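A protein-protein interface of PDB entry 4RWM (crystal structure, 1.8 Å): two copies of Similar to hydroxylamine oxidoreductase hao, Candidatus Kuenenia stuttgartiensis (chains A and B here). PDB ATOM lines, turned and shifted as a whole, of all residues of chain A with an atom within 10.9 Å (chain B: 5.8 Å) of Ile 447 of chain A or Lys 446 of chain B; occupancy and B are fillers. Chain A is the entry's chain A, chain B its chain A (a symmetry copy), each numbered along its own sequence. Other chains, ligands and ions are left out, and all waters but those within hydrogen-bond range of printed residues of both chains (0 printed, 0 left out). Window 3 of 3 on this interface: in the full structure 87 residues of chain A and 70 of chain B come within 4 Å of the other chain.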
ATOM      1  N   ARG A 439     -18.187  28.557 -37.048  1.00  0.00           N
ATOM      2  CA  ARG A 439     -16.978  27.772 -36.773  1.00  0.00           C
ATOM      3  C   ARG A 439     -17.036  27.079 -35.415  1.00  0.00           C
ATOM      4  O   ARG A 439     -16.642  25.912 -35.304  1.00  0.00           O
ATOM      5  CB  ARG A 439     -15.711  28.623 -36.873  1.00  0.00           C
ATOM      6  CG  ARG A 439     -15.320  28.964 -38.293  1.00  0.00           C
ATOM      7  CD  ARG A 439     -14.057  29.805 -38.345  1.00  0.00           C
ATOM      8  NE  ARG A 439     -12.836  29.005 -38.459  1.00  0.00           N
ATOM      9  CZ  ARG A 439     -11.618  29.524 -38.627  1.00  0.00           C
ATOM     10  NH1 ARG A 439     -11.443  30.843 -38.680  1.00  0.00           N
ATOM     11  NH2 ARG A 439     -10.565  28.728 -38.737  1.00  0.00           N
ATOM     12  N   PHE A 440     -17.519  27.784 -34.390  1.00  0.00           N
ATOM     13  CA  PHE A 440     -17.724  27.173 -33.071  1.00  0.00           C
ATOM     14  C   PHE A 440     -18.716  26.010 -33.144  1.00  0.00           C
ATOM     15  O   PHE A 440     -18.470  24.940 -32.579  1.00  0.00           O
ATOM     16  CB  PHE A 440     -18.253  28.183 -32.043  1.00  0.00           C
ATOM     17  CG  PHE A 440     -17.184  28.964 -31.318  1.00  0.00           C
ATOM     18  CD1 PHE A 440     -16.141  28.316 -30.662  1.00  0.00           C
ATOM     19  CD2 PHE A 440     -17.255  30.351 -31.242  1.00  0.00           C
ATOM     20  CE1 PHE A 440     -15.168  29.038 -29.983  1.00  0.00           C
ATOM     21  CE2 PHE A 440     -16.289  31.077 -30.563  1.00  0.00           C
ATOM     22  CZ  PHE A 440     -15.244  30.421 -29.928  1.00  0.00           C
ATOM     23  N   ALA A 441     -19.843  26.229 -33.818  1.00  0.00           N
ATOM     24  CA  ALA A 441     -20.886  25.202 -33.927  1.00  0.00           C
ATOM     25  C   ALA A 441     -20.388  23.949 -34.661  1.00  0.00           C
ATOM     26  O   ALA A 441     -20.710  22.823 -34.265  1.00  0.00           O
ATOM     27  CB  ALA A 441     -22.130  25.764 -34.614  1.00  0.00           C
ATOM     28  N   ALA A 442     -19.598  24.146 -35.715  1.00  0.00           N
ATOM     29  CA  ALA A 442     -19.051  23.026 -36.490  1.00  0.00           C
ATOM     30  C   ALA A 442     -18.064  22.189 -35.666  1.00  0.00           C
ATOM     31  O   ALA A 442     -18.089  20.952 -35.724  1.00  0.00           O
ATOM     32  CB  ALA A 442     -18.385  23.533 -37.765  1.00  0.00           C
ATOM     33  N   ILE A 443     -17.209  22.864 -34.898  1.00  0.00           N
ATOM     34  CA  ILE A 443     -16.262  22.197 -34.005  1.00  0.00           C
ATOM     35  C   ILE A 443     -16.995  21.423 -32.910  1.00  0.00           C
ATOM     36  O   ILE A 443     -16.717  20.245 -32.673  1.00  0.00           O
ATOM     37  CB  ILE A 443     -15.290  23.210 -33.351  1.00  0.00           C
ATOM     38  CG1 ILE A 443     -14.284  23.724 -34.382  1.00  0.00           C
ATOM     39  CG2 ILE A 443     -14.546  22.580 -32.177  1.00  0.00           C
ATOM     40  CD1 ILE A 443     -13.497  24.937 -33.915  1.00  0.00           C
ATOM     41  N   GLU A 444     -17.938  22.090 -32.252  1.00  0.00           N
ATOM     42  CA  GLU A 444     -18.687  21.479 -31.154  1.00  0.00           C
ATOM     43  C   GLU A 444     -19.507  20.263 -31.606  1.00  0.00           C
ATOM     44  O   GLU A 444     -19.609  19.277 -30.874  1.00  0.00           O
ATOM     45  CB  GLU A 444     -19.567  22.527 -30.464  1.00  0.00           C
ATOM     46  CG  GLU A 444     -18.744  23.557 -29.667  1.00  0.00           C
ATOM     47  CD  GLU A 444     -19.519  24.820 -29.302  1.00  0.00           C
ATOM     48  OE1 GLU A 444     -18.961  25.663 -28.564  1.00  0.00           O
ATOM     49  OE2 GLU A 444     -20.676  24.977 -29.748  1.00  0.00           O
ATOM     50  N   LYS A 445     -20.073  20.326 -32.808  1.00  0.00           N
ATOM     51  CA  LYS A 445     -20.781  19.179 -33.378  1.00  0.00           C
ATOM     52  C   LYS A 445     -19.825  18.005 -33.619  1.00  0.00           C
ATOM     53  O   LYS A 445     -20.121  16.877 -33.232  1.00  0.00           O
ATOM     54  CB  LYS A 445     -21.481  19.556 -34.688  1.00  0.00           C
ATOM     55  CG  LYS A 445     -22.427  18.474 -35.216  1.00  0.00           C
ATOM     56  CD  LYS A 445     -22.876  18.751 -36.638  1.00  0.00           C
ATOM     57  CE  LYS A 445     -23.715  17.597 -37.184  1.00  0.00           C
ATOM     58  NZ  LYS A 445     -24.047  17.787 -38.620  1.00  0.00           N
ATOM     59  N   LYS A 446     -18.677  18.276 -34.237  1.00  0.00           N
ATOM     60  CA  LYS A 446     -17.719  17.222 -34.586  1.00  0.00           C
ATOM     61  C   LYS A 446     -17.157  16.491 -33.365  1.00  0.00           C
ATOM     62  O   LYS A 446     -16.956  15.275 -33.412  1.00  0.00           O
ATOM     63  CB  LYS A 446     -16.564  17.785 -35.429  1.00  0.00           C
ATOM     64  CG  LYS A 446     -15.638  16.714 -36.002  1.00  0.00           C
ATOM     65  CD  LYS A 446     -14.578  17.301 -36.916  1.00  0.00           C
ATOM     66  CE  LYS A 446     -13.577  16.237 -37.367  1.00  0.00           C
ATOM     67  NZ  LYS A 446     -14.188  15.213 -38.255  1.00  0.00           N
ATOM     68  N   ILE A 447     -16.904  17.224 -32.282  1.00  0.00           N
ATOM     69  CA  ILE A 447     -16.338  16.629 -31.064  1.00  0.00           C
ATOM     70  C   ILE A 447     -17.398  16.200 -30.035  1.00  0.00           C
ATOM     71  O   ILE A 447     -17.056  15.640 -28.991  1.00  0.00           O
ATOM     72  CB  ILE A 447     -15.309  17.579 -30.388  1.00  0.00           C
ATOM     73  CG1 ILE A 447     -16.000  18.753 -29.679  1.00  0.00           C
ATOM     74  CG2 ILE A 447     -14.300  18.083 -31.415  1.00  0.00           C
ATOM     75  CD1 ILE A 447     -15.028  19.731 -29.046  1.00  0.00           C
ATOM     76  N   GLY A 448     -18.670  16.466 -30.323  1.00  0.00           N
ATOM     77  CA  GLY A 448     -19.764  16.080 -29.431  1.00  0.00           C
ATOM     78  C   GLY A 448     -19.835  16.879 -28.140  1.00  0.00           C
ATOM     79  O   GLY A 448     -20.240  16.352 -27.100  1.00  0.00           O
ATOM     80  N   LEU A 449     -19.442  18.151 -28.197  1.00  0.00           N
ATOM     81  CA  LEU A 449     -19.566  19.048 -27.051  1.00  0.00           C
ATOM     82  C   LEU A 449     -20.931  19.729 -27.113  1.00  0.00           C
ATOM     83  O   LEU A 449     -21.264  20.365 -28.111  1.00  0.00           O
ATOM     84  CB  LEU A 449     -18.445  20.091 -27.063  1.00  0.00           C
ATOM     85  CG  LEU A 449     -18.300  20.973 -25.814  1.00  0.00           C
ATOM     86  CD1 LEU A 449     -16.897  21.553 -25.722  1.00  0.00           C
ATOM     87  CD2 LEU A 449     -19.338  22.090 -25.796  1.00  0.00           C
ATOM     88  N   GLU A 450     -21.721  19.580 -26.051  1.00  0.00           N
ATOM     89  CA  GLU A 450     -23.035  20.210 -25.974  1.00  0.00           C
ATOM     90  C   GLU A 450     -22.886  21.587 -25.339  1.00  0.00           C
ATOM     91  O   GLU A 450     -22.758  21.713 -24.119  1.00  0.00           O
ATOM     92  CB  GLU A 450     -24.016  19.351 -25.169  1.00  0.00           C
ATOM     93  CG  GLU A 450     -25.448  19.897 -25.166  1.00  0.00           C
ATOM     94  CD  GLU A 450     -26.429  19.000 -24.422  1.00  0.00           C
ATOM     95  OE1 GLU A 450     -27.260  19.539 -23.654  1.00  0.00           O
ATOM     96  OE2 GLU A 450     -26.371  17.759 -24.604  1.00  0.00           O
ATOM     97  N   HIS A 451     -22.896  22.617 -26.179  1.00  0.00           N
ATOM     98  CA  HIS A 451     -22.712  23.983 -25.709  1.00  0.00           C
ATOM     99  C   HIS A 451     -23.984  24.495 -25.048  1.00  0.00           C
ATOM    100  O   HIS A 451     -25.077  24.339 -25.591  1.00  0.00           O
ATOM    101  CB  HIS A 451     -22.315  24.900 -26.870  1.00  0.00           C
ATOM    102  CG  HIS A 451     -22.359  26.357 -26.529  1.00  0.00           C
ATOM    103  ND1 HIS A 451     -21.460  26.945 -25.666  1.00  0.00           N
ATOM    104  CD2 HIS A 451     -23.201  27.341 -26.926  1.00  0.00           C
ATOM    105  CE1 HIS A 451     -21.743  28.233 -25.550  1.00  0.00           C
ATOM    106  NE2 HIS A 451     -22.796  28.497 -26.305  1.00  0.00           N
ATOM    107  N   ALA B 441     -12.081  27.810 -24.445  1.00  0.00           N
ATOM    108  CA  ALA B 441     -11.517  27.073 -23.308  1.00  0.00           C
ATOM    109  C   ALA B 441     -12.184  25.704 -23.118  1.00  0.00           C
ATOM    110  O   ALA B 441     -11.506  24.714 -22.820  1.00  0.00           O
ATOM    111  CB  ALA B 441     -11.619  27.898 -22.024  1.00  0.00           C
ATOM    112  N   ALA B 442     -13.501  25.648 -23.301  1.00  0.00           N
ATOM    113  CA  ALA B 442     -14.249  24.393 -23.160  1.00  0.00           C
ATOM    114  C   ALA B 442     -13.863  23.373 -24.238  1.00  0.00           C
ATOM    115  O   ALA B 442     -13.701  22.180 -23.945  1.00  0.00           O
ATOM    116  CB  ALA B 442     -15.751  24.658 -23.190  1.00  0.00           C
ATOM    117  N   ILE B 443     -13.710  23.845 -25.475  1.00  0.00           N
ATOM    118  CA  ILE B 443     -13.273  23.002 -26.588  1.00  0.00           C
ATOM    119  C   ILE B 443     -11.852  22.487 -26.359  1.00  0.00           C
ATOM    120  O   ILE B 443     -11.585  21.289 -26.480  1.00  0.00           O
ATOM    121  CB  ILE B 443     -13.328  23.768 -27.934  1.00  0.00           C
ATOM    122  CG1 ILE B 443     -14.779  23.965 -28.374  1.00  0.00           C
ATOM    123  CG2 ILE B 443     -12.558  23.024 -29.021  1.00  0.00           C
ATOM    124  CD1 ILE B 443     -14.943  24.961 -29.510  1.00  0.00           C
ATOM    125  N   GLU B 444     -10.946  23.399 -26.019  1.00  0.00           N
ATOM    126  CA  GLU B 444      -9.542  23.046 -25.810  1.00  0.00           C
ATOM    127  C   GLU B 444      -9.350  22.056 -24.653  1.00  0.00           C
ATOM    128  O   GLU B 444      -8.507  21.161 -24.736  1.00  0.00           O
ATOM    129  CB  GLU B 444      -8.700  24.311 -25.614  1.00  0.00           C
ATOM    130  CG  GLU B 444      -8.564  25.136 -26.908  1.00  0.00           C
ATOM    131  CD  GLU B 444      -8.088  26.568 -26.682  1.00  0.00           C
ATOM    132  OE1 GLU B 444      -7.848  27.277 -27.686  1.00  0.00           O
ATOM    133  OE2 GLU B 444      -7.955  26.991 -25.514  1.00  0.00           O
ATOM    134  N   LYS B 445     -10.136  22.205 -23.591  1.00  0.00           N
ATOM    135  CA  LYS B 445     -10.110  21.248 -22.483  1.00  0.00           C
ATOM    136  C   LYS B 445     -10.578  19.862 -22.942  1.00  0.00           C
ATOM    137  O   LYS B 445      -9.920  18.863 -22.661  1.00  0.00           O
ATOM    138  CB  LYS B 445     -10.978  21.730 -21.316  1.00  0.00           C
ATOM    139  CG  LYS B 445     -10.815  20.898 -20.041  1.00  0.00           C
ATOM    140  CD  LYS B 445     -11.881  21.214 -19.010  1.00  0.00           C
ATOM    141  CE  LYS B 445     -11.772  20.285 -17.803  1.00  0.00           C
ATOM    142  NZ  LYS B 445     -12.892  20.488 -16.847  1.00  0.00           N
ATOM    143  N   LYS B 446     -11.698  19.808 -23.659  1.00  0.00           N
ATOM    144  CA  LYS B 446     -12.281  18.533 -24.089  1.00  0.00           C
ATOM    145  C   LYS B 446     -11.368  17.740 -25.026  1.00  0.00           C
ATOM    146  O   LYS B 446     -11.306  16.511 -24.933  1.00  0.00           O
ATOM    147  CB  LYS B 446     -13.647  18.748 -24.758  1.00  0.00           C
ATOM    148  CG  LYS B 446     -14.406  17.454 -25.047  1.00  0.00           C
ATOM    149  CD  LYS B 446     -15.793  17.715 -25.604  1.00  0.00           C
ATOM    150  CE  LYS B 446     -16.482  16.414 -26.018  1.00  0.00           C
ATOM    151  NZ  LYS B 446     -16.798  15.537 -24.859  1.00  0.00           N
ATOM    152  N   ILE B 447     -10.667  18.433 -25.921  1.00  0.00           N
ATOM    153  CA  ILE B 447      -9.780  17.771 -26.887  1.00  0.00           C
ATOM    154  C   ILE B 447      -8.320  17.668 -26.417  1.00  0.00           C
ATOM    155  O   ILE B 447      -7.484  17.088 -27.113  1.00  0.00           O
ATOM    156  CB  ILE B 447      -9.833  18.461 -28.279  1.00  0.00           C
ATOM    157  CG1 ILE B 447      -9.084  19.802 -28.278  1.00  0.00           C
ATOM    158  CG2 ILE B 447     -11.281  18.648 -28.723  1.00  0.00           C
ATOM    159  CD1 ILE B 447      -9.152  20.531 -29.606  1.00  0.00           C
ATOM    160  N   GLY B 448      -8.013  18.232 -25.251  1.00  0.00           N
ATOM    161  CA  GLY B 448      -6.663  18.175 -24.692  1.00  0.00           C
ATOM    162  C   GLY B 448      -5.639  19.022 -25.429  1.00  0.00           C
ATOM    163  O   GLY B 448      -4.462  18.662 -25.499  1.00  0.00           O
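Of the 8 printed residues of chain B, 4 touch a printed residue of chain A.
Hydrophobic or aromatic side chains of chain B within 4 Å of the printed part of chain A: Ile 443 and Ile 447.
Of the 13 printed residues of chain A, 5 touch a printed residue of chain B.
Hydrophobic or aromatic side chains of chain A that line the printed part of chain B: Phe 440, Ile 443, Ile 447 and Leu 449.
Among the printed residues, pairs that only touch across the chains: Phe 440 of chain A with Ile 443 of chain B, Ile 443 of chain A with Ile 443 of chain B, Ile 447 of chain A with Lys 446 of chain B, Ile 447 of chain A with Ile 447 of chain B, Gly 448 of chain A with Lys 446 of chain B, Leu 449 of chain A with Ala 442 of chain B, Leu 449 of chain A with Ile 443 of chain B and Leu 449 of chain A with Lys 446 of chain B.
Of chain B, only Lys 446 and Ile 447 come within 4 Å of Ile 447 of chain A.
Lys 446 of chain B touches three residues of chain A.
Of chain A, only Leu 449 comes within 4 Å of Ala 442 of chain B.
Printed residues of chain A within 4 Å of Ile 443 of chain B: Phe 440, Ile 443 and Leu 449.
Of the printed residues of chain B, Ile 443 of chain A touches Ile 443 (3.6 Å).
Printed residues of chain B within 4 Å of Leu 449 of chain A: Ala 442 (3.7 Å), Ile 443 (3.9 Å) and Lys 446 (3.8 Å).
The nearest residue of chain B that does not touch Ile 447 of chain A is Ile 443 of chain B (4.1 Å).
The nearest residue of chain A that does not touch Lys 446 of chain B is Glu 450 of chain A (6.1 Å).
The backbone NH (N) of Leu 449 of chain A is in hydrogen-bond range of the backbone carbonyl oxygen (O) of Glu 444 of chain A, at 2.9 Å.
Ile 443 of chain A touches its own counterpart, Ile 443 of chain B.
Ile 447 of chain A touches Lys 446 of chain B, but with the chains exchanged Lys 446 of chain A does not touch Ile 447 of chain B (7.8 Å).
Ile 447 of chain B touches its own counterpart, Ile 447 of chain A.
Gly 448 of chain A touches Lys 446 of chain B, but with the chains exchanged Lys 446 of chain A does not touch Gly 448 of chain B (12.3 Å).
Of the 8 pairs that touch across the chains among the printed residues, 2 have their exchanged pair printed and touching as well.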
